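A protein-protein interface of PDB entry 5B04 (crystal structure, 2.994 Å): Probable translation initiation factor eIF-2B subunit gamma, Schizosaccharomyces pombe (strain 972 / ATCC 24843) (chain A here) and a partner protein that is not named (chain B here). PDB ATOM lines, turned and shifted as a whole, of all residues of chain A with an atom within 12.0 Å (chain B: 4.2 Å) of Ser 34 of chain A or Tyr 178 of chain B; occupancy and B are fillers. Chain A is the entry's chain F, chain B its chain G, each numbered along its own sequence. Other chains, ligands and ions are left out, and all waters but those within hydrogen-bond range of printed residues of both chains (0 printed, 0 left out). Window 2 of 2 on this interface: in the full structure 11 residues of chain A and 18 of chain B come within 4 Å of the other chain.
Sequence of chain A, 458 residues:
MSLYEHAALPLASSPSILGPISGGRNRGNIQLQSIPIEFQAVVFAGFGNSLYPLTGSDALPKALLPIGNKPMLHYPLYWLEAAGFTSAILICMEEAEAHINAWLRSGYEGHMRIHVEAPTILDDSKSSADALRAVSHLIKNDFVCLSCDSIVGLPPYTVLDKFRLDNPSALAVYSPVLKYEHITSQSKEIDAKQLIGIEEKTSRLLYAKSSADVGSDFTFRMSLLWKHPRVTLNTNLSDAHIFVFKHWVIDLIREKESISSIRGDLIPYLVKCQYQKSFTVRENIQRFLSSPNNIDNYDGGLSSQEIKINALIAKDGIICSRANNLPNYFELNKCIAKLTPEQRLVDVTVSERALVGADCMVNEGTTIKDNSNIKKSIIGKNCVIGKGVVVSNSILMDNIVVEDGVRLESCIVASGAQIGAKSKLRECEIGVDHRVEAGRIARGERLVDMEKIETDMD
Among the printed residues, merely in contact across the chains: Ser 34 of chain A with Tyr 178 of chain B, Pro 36 of chain A with Asp 177 of chain B and Ser 34 of chain A with His 193 of chain B.
The backbone carbonyl oxygen (O) of Ser 34 of chain A sits close to the backbone carbonyl oxygen (O) of Asp 177 of chain B (2.9 Å). OG of Ser 34 of chain A lies within hydrogen-bond range of N of Gln 179 of chain B (3.4 Å).
OH of Tyr 178 of chain B sits at hydrogen-bond distance from ND1 of His 189 of chain B. The backbone NH of Leu 190 of chain B lies within hydrogen-bond range of the side-chain hydroxyl of Tyr 178 of chain B, at 3.5 Å.
Hydrophobic or aromatic side chains of chain B that line the printed part of chain A: Tyr 178 and His 193. Printed residues of chain A that touch a printed residue of chain B: Ser 34 and Pro 36. Hydrophobic or aromatic side chains of chain A within 4 Å of the printed part of chain B: Pro 36. Among the printed residues, 5 pairs touch across the chains.
Of the printed residues of chain B, Pro 36 of chain A touches Asp 177. Ile 37 of chain A touches none of the printed residues of chain B. Asn 141 of chain A touches none of the printed residues of chain B. No residue of chain A comes within 4 Å of Val 174 of chain B. No residue of chain A comes within 4 Å of Ile 175 of chain B. Of the printed residues of chain A, Asp 177 of chain B touches Ser 34 and Pro 36. Of chain A, only Ser 34 comes within 4 Å of Tyr 178 of chain B. No residue of chain A comes within 4 Å of Thr 180 of chain B. No residue of chain A comes within 4 Å of Pro 181 of chain B. No residue of chain A comes within 4 Å of Leu 186 of chain B. No residue of chain A comes within 4 Å of His 189 of chain B. The nearest printed residue of chain B that does not touch Ser 34 of chain A is Val 174 of chain B (5.3 Å). The nearest residue of chain A that does not touch Tyr 178 of chain B is Leu 32 of chain A (6.0 Å). The nearest printed residue of chain B that does not touch Pro 36 of chain A is Tyr 178 of chain B (6.9 Å).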
ATOM      1  N   LEU A  32       4.121 -21.151 -29.636  1.00  0.00           N
ATOM      2  CA  LEU A  32       3.218 -21.001 -30.774  1.00  0.00           C
ATOM      3  C   LEU A  32       2.097 -22.031 -30.730  1.00  0.00           C
ATOM      4  O   LEU A  32       0.925 -21.715 -30.921  1.00  0.00           O
ATOM      5  CB  LEU A  32       3.999 -21.105 -32.096  1.00  0.00           C
ATOM      6  CG  LEU A  32       5.140 -22.105 -32.345  1.00  0.00           C
ATOM      7  CD1 LEU A  32       4.696 -23.558 -32.521  1.00  0.00           C
ATOM      8  CD2 LEU A  32       5.936 -21.653 -33.559  1.00  0.00           C
ATOM      9  N   GLN A  33       2.494 -23.266 -30.457  1.00  0.00           N
ATOM     10  CA  GLN A  33       1.626 -24.428 -30.416  1.00  0.00           C
ATOM     11  C   GLN A  33       2.259 -25.249 -29.318  1.00  0.00           C
ATOM     12  O   GLN A  33       2.168 -26.478 -29.281  1.00  0.00           O
ATOM     13  CB  GLN A  33       1.568 -25.119 -31.775  1.00  0.00           C
ATOM     14  CG  GLN A  33       0.566 -24.514 -32.737  1.00  0.00           C
ATOM     15  CD  GLN A  33      -0.858 -24.950 -32.465  1.00  0.00           C
ATOM     16  OE1 GLN A  33      -1.340 -25.909 -33.070  1.00  0.00           O
ATOM     17  NE2 GLN A  33      -1.544 -24.246 -31.573  1.00  0.00           N
ATOM     18  N   SER A  34       2.949 -24.523 -28.444  1.00  0.00           N
ATOM     19  CA  SER A  34       3.461 -25.054 -27.196  1.00  0.00           C
ATOM     20  C   SER A  34       2.276 -25.513 -26.355  1.00  0.00           C
ATOM     21  O   SER A  34       2.379 -26.407 -25.518  1.00  0.00           O
ATOM     22  CB  SER A  34       4.319 -24.010 -26.482  1.00  0.00           C
ATOM     23  OG  SER A  34       5.474 -23.695 -27.242  1.00  0.00           O
ATOM     24  N   ILE A  35       1.142 -24.871 -26.611  1.00  0.00           N
ATOM     25  CA  ILE A  35      -0.099 -25.162 -25.916  1.00  0.00           C
ATOM     26  C   ILE A  35      -0.820 -26.428 -26.376  1.00  0.00           C
ATOM     27  O   ILE A  35      -1.115 -26.594 -27.560  1.00  0.00           O
ATOM     28  CB  ILE A  35      -1.036 -23.943 -26.062  1.00  0.00           C
ATOM     29  CG1 ILE A  35      -1.205 -23.565 -27.536  1.00  0.00           C
ATOM     30  CG2 ILE A  35      -0.474 -22.754 -25.307  1.00  0.00           C
ATOM     31  CD1 ILE A  35      -2.144 -22.407 -27.768  1.00  0.00           C
ATOM     32  N   PRO A  36      -1.082 -27.344 -25.434  1.00  0.00           N
ATOM     33  CA  PRO A  36      -1.870 -28.549 -25.705  1.00  0.00           C
ATOM     34  C   PRO A  36      -3.356 -28.227 -25.811  1.00  0.00           C
ATOM     35  O   PRO A  36      -3.752 -27.085 -25.574  1.00  0.00           O
ATOM     36  CB  PRO A  36      -1.582 -29.434 -24.491  1.00  0.00           C
ATOM     37  CG  PRO A  36      -1.282 -28.468 -23.399  1.00  0.00           C
ATOM     38  CD  PRO A  36      -0.563 -27.322 -24.055  1.00  0.00           C
ATOM     39  N   ILE A  37      -4.164 -29.219 -26.162  1.00  0.00           N
ATOM     40  CA  ILE A  37      -5.602 -29.015 -26.272  1.00  0.00           C
ATOM     41  C   ILE A  37      -6.280 -29.204 -24.918  1.00  0.00           C
ATOM     42  O   ILE A  37      -6.176 -30.265 -24.304  1.00  0.00           O
ATOM     43  CB  ILE A  37      -6.233 -29.971 -27.298  1.00  0.00           C
ATOM     44  CG1 ILE A  37      -5.569 -29.794 -28.666  1.00  0.00           C
ATOM     45  CG2 ILE A  37      -7.731 -29.732 -27.398  1.00  0.00           C
ATOM     46  CD1 ILE A  37      -6.199 -30.622 -29.765  1.00  0.00           C
ATOM     47  N   GLU A  38      -6.968 -28.163 -24.458  1.00  0.00           N
ATOM     48  CA  GLU A  38      -7.665 -28.208 -23.178  1.00  0.00           C
ATOM     49  C   GLU A  38      -9.031 -28.869 -23.332  1.00  0.00           C
ATOM     50  O   GLU A  38      -9.384 -29.773 -22.574  1.00  0.00           O
ATOM     51  CB  GLU A  38      -7.817 -26.799 -22.601  1.00  0.00           C
ATOM     52  CG  GLU A  38      -8.324 -26.760 -21.169  1.00  0.00           C
ATOM     53  CD  GLU A  38      -8.436 -25.348 -20.629  1.00  0.00           C
ATOM     54  OE1 GLU A  38      -8.193 -24.394 -21.399  1.00  0.00           O
ATOM     55  OE2 GLU A  38      -8.761 -25.190 -19.432  1.00  0.00           O
ATOM     56  N   ASN A 141      -9.393 -35.582 -24.654  1.00  0.00           N
ATOM     57  CA  ASN A 141      -9.283 -34.571 -23.608  1.00  0.00           C
ATOM     58  C   ASN A 141     -10.615 -34.354 -22.904  1.00  0.00           C
ATOM     59  O   ASN A 141     -11.572 -35.093 -23.136  1.00  0.00           O
ATOM     60  CB  ASN A 141      -8.785 -33.247 -24.191  1.00  0.00           C
ATOM     61  CG  ASN A 141      -7.554 -33.415 -25.060  1.00  0.00           C
ATOM     62  OD1 ASN A 141      -7.507 -32.929 -26.190  1.00  0.00           O
ATOM     63  ND2 ASN A 141      -6.551 -34.108 -24.536  1.00  0.00           N
ATOM     64  N   VAL B 174       4.439 -25.837 -18.397  1.00  0.00           N
ATOM     65  CA  VAL B 174       4.648 -24.906 -19.497  1.00  0.00           C
ATOM     66  C   VAL B 174       5.865 -25.308 -20.321  1.00  0.00           C
ATOM     67  O   VAL B 174       5.767 -25.494 -21.531  1.00  0.00           O
ATOM     68  CB  VAL B 174       4.834 -23.462 -18.992  1.00  0.00           C
ATOM     69  CG1 VAL B 174       5.307 -22.557 -20.120  1.00  0.00           C
ATOM     70  CG2 VAL B 174       3.543 -22.944 -18.388  1.00  0.00           C
ATOM     71  N   ILE B 175       7.004 -25.455 -19.652  1.00  0.00           N
ATOM     72  CA  ILE B 175       8.251 -25.814 -20.317  1.00  0.00           C
ATOM     73  C   ILE B 175       8.202 -27.243 -20.865  1.00  0.00           C
ATOM     74  O   ILE B 175       8.721 -27.518 -21.949  1.00  0.00           O
ATOM     75  CB  ILE B 175       9.458 -25.652 -19.360  1.00  0.00           C
ATOM     76  CG1 ILE B 175       9.721 -24.167 -19.096  1.00  0.00           C
ATOM     77  CG2 ILE B 175      10.707 -26.300 -19.933  1.00  0.00           C
ATOM     78  CD1 ILE B 175      10.844 -23.907 -18.117  1.00  0.00           C
ATOM     79  N   GLN B 176       7.558 -28.144 -20.127  1.00  0.00           N
ATOM     80  CA  GLN B 176       7.431 -29.534 -20.561  1.00  0.00           C
ATOM     81  C   GLN B 176       6.645 -29.644 -21.865  1.00  0.00           C
ATOM     82  O   GLN B 176       7.036 -30.376 -22.774  1.00  0.00           O
ATOM     83  CB  GLN B 176       6.759 -30.382 -19.476  1.00  0.00           C
ATOM     84  CG  GLN B 176       6.604 -31.850 -19.838  1.00  0.00           C
ATOM     85  CD  GLN B 176       7.927 -32.590 -19.860  1.00  0.00           C
ATOM     86  OE1 GLN B 176       8.696 -32.484 -20.815  1.00  0.00           O
ATOM     87  NE2 GLN B 176       8.198 -33.347 -18.803  1.00  0.00           N
ATOM     88  N   ASP B 177       5.538 -28.912 -21.954  1.00  0.00           N
ATOM     89  CA  ASP B 177       4.711 -28.918 -23.156  1.00  0.00           C
ATOM     90  C   ASP B 177       5.302 -27.967 -24.194  1.00  0.00           C
ATOM     91  O   ASP B 177       4.871 -27.948 -25.346  1.00  0.00           O
ATOM     92  CB  ASP B 177       3.264 -28.547 -22.821  1.00  0.00           C
ATOM     93  CG  ASP B 177       2.521 -29.670 -22.126  1.00  0.00           C
ATOM     94  OD1 ASP B 177       2.949 -30.837 -22.251  1.00  0.00           O
ATOM     95  OD2 ASP B 177       1.503 -29.386 -21.459  1.00  0.00           O
ATOM     96  N   TYR B 178       6.288 -27.179 -23.776  1.00  0.00           N
ATOM     97  CA  TYR B 178       6.923 -26.208 -24.663  1.00  0.00           C
ATOM     98  C   TYR B 178       7.701 -26.854 -25.802  1.00  0.00           C
ATOM     99  O   TYR B 178       8.579 -27.687 -25.572  1.00  0.00           O
ATOM    100  CB  TYR B 178       7.860 -25.300 -23.864  1.00  0.00           C
ATOM    101  CG  TYR B 178       8.633 -24.310 -24.700  1.00  0.00           C
ATOM    102  CD1 TYR B 178       8.027 -23.161 -25.192  1.00  0.00           C
ATOM    103  CD2 TYR B 178       9.975 -24.515 -24.984  1.00  0.00           C
ATOM    104  CE1 TYR B 178       8.735 -22.250 -25.953  1.00  0.00           C
ATOM    105  CE2 TYR B 178      10.689 -23.612 -25.742  1.00  0.00           C
ATOM    106  CZ  TYR B 178      10.067 -22.482 -26.224  1.00  0.00           C
ATOM    107  OH  TYR B 178      10.781 -21.581 -26.980  1.00  0.00           O
ATOM    108  N   GLN B 179       7.375 -26.465 -27.031  1.00  0.00           N
ATOM    109  CA  GLN B 179       8.030 -27.030 -28.204  1.00  0.00           C
ATOM    110  C   GLN B 179       8.946 -26.025 -28.892  1.00  0.00           C
ATOM    111  O   GLN B 179       8.532 -24.916 -29.234  1.00  0.00           O
ATOM    112  CB  GLN B 179       7.032 -27.600 -29.213  1.00  0.00           C
ATOM    113  CG  GLN B 179       7.001 -29.116 -29.235  1.00  0.00           C
ATOM    114  CD  GLN B 179       8.389 -29.719 -29.345  1.00  0.00           C
ATOM    115  OE1 GLN B 179       8.789 -30.539 -28.519  1.00  0.00           O
ATOM    116  NE2 GLN B 179       9.132 -29.313 -30.369  1.00  0.00           N
ATOM    117  N   THR B 180      10.193 -26.434 -29.095  1.00  0.00           N
ATOM    118  CA  THR B 180      11.200 -25.588 -29.719  1.00  0.00           C
ATOM    119  C   THR B 180      10.937 -25.383 -31.206  1.00  0.00           C
ATOM    120  O   THR B 180      10.761 -26.351 -31.947  1.00  0.00           O
ATOM    121  CB  THR B 180      12.612 -26.187 -29.551  1.00  0.00           C
ATOM    122  OG1 THR B 180      12.784 -26.660 -28.209  1.00  0.00           O
ATOM    123  CG2 THR B 180      13.679 -25.151 -29.871  1.00  0.00           C
ATOM    124  N   PRO B 181      10.896 -24.117 -31.647  1.00  0.00           N
ATOM    125  CA  PRO B 181      10.929 -23.835 -33.082  1.00  0.00           C
ATOM    126  C   PRO B 181      12.365 -23.937 -33.567  1.00  0.00           C
ATOM    127  O   PRO B 181      13.265 -23.652 -32.782  1.00  0.00           O
ATOM    128  CB  PRO B 181      10.402 -22.404 -33.170  1.00  0.00           C
ATOM    129  CG  PRO B 181      10.828 -21.786 -31.879  1.00  0.00           C
ATOM    130  CD  PRO B 181      10.777 -22.888 -30.843  1.00  0.00           C
ATOM    131  N   LEU B 186      16.389 -23.396 -27.868  1.00  0.00           N
ATOM    132  CA  LEU B 186      15.846 -23.317 -26.511  1.00  0.00           C
ATOM    133  C   LEU B 186      16.173 -22.073 -25.674  1.00  0.00           C
ATOM    134  O   LEU B 186      15.302 -21.562 -24.969  1.00  0.00           O
ATOM    135  CB  LEU B 186      16.296 -24.557 -25.733  1.00  0.00           C
ATOM    136  CG  LEU B 186      15.747 -24.758 -24.320  1.00  0.00           C
ATOM    137  CD1 LEU B 186      14.237 -24.637 -24.308  1.00  0.00           C
ATOM    138  CD2 LEU B 186      16.176 -26.109 -23.774  1.00  0.00           C
ATOM    139  N   HIS B 189      14.491 -18.242 -26.812  1.00  0.00           N
ATOM    140  CA  HIS B 189      13.048 -18.090 -26.981  1.00  0.00           C
ATOM    141  C   HIS B 189      12.185 -18.687 -25.864  1.00  0.00           C
ATOM    142  O   HIS B 189      10.989 -18.390 -25.784  1.00  0.00           O
ATOM    143  CB  HIS B 189      12.601 -18.683 -28.318  1.00  0.00           C
ATOM    144  CG  HIS B 189      11.197 -18.321 -28.681  1.00  0.00           C
ATOM    145  ND1 HIS B 189      10.104 -19.096 -28.343  1.00  0.00           N
ATOM    146  CD2 HIS B 189      10.695 -17.212 -29.274  1.00  0.00           C
ATOM    147  CE1 HIS B 189       9.002 -18.507 -28.764  1.00  0.00           C
ATOM    148  NE2 HIS B 189       9.332 -17.356 -29.330  1.00  0.00           N
ATOM    149  N   LEU B 190      12.760 -19.525 -25.007  1.00  0.00           N
ATOM    150  CA  LEU B 190      11.979 -20.057 -23.893  1.00  0.00           C
ATOM    151  C   LEU B 190      11.656 -18.939 -22.912  1.00  0.00           C
ATOM    152  O   LEU B 190      10.583 -18.920 -22.313  1.00  0.00           O
ATOM    153  CB  LEU B 190      12.710 -21.198 -23.179  1.00  0.00           C
ATOM    154  CG  LEU B 190      11.979 -21.817 -21.977  1.00  0.00           C
ATOM    155  CD1 LEU B 190      10.534 -22.179 -22.304  1.00  0.00           C
ATOM    156  CD2 LEU B 190      12.717 -23.033 -21.430  1.00  0.00           C
ATOM    157  N   HIS B 193       8.553 -16.932 -24.257  1.00  0.00           N
ATOM    158  CA  HIS B 193       7.299 -17.653 -24.076  1.00  0.00           C
ATOM    159  C   HIS B 193       6.866 -17.605 -22.615  1.00  0.00           C
ATOM    160  O   HIS B 193       5.685 -17.439 -22.311  1.00  0.00           O
ATOM    161  CB  HIS B 193       7.442 -19.101 -24.544  1.00  0.00           C
ATOM    162  CG  HIS B 193       6.157 -19.871 -24.534  1.00  0.00           C
ATOM    163  ND1 HIS B 193       5.980 -21.011 -23.780  1.00  0.00           N
ATOM    164  CD2 HIS B 193       4.989 -19.665 -25.186  1.00  0.00           C
ATOM    165  CE1 HIS B 193       4.757 -21.475 -23.969  1.00  0.00           C
ATOM    166  NE2 HIS B 193       4.135 -20.675 -24.817  1.00  0.00           N
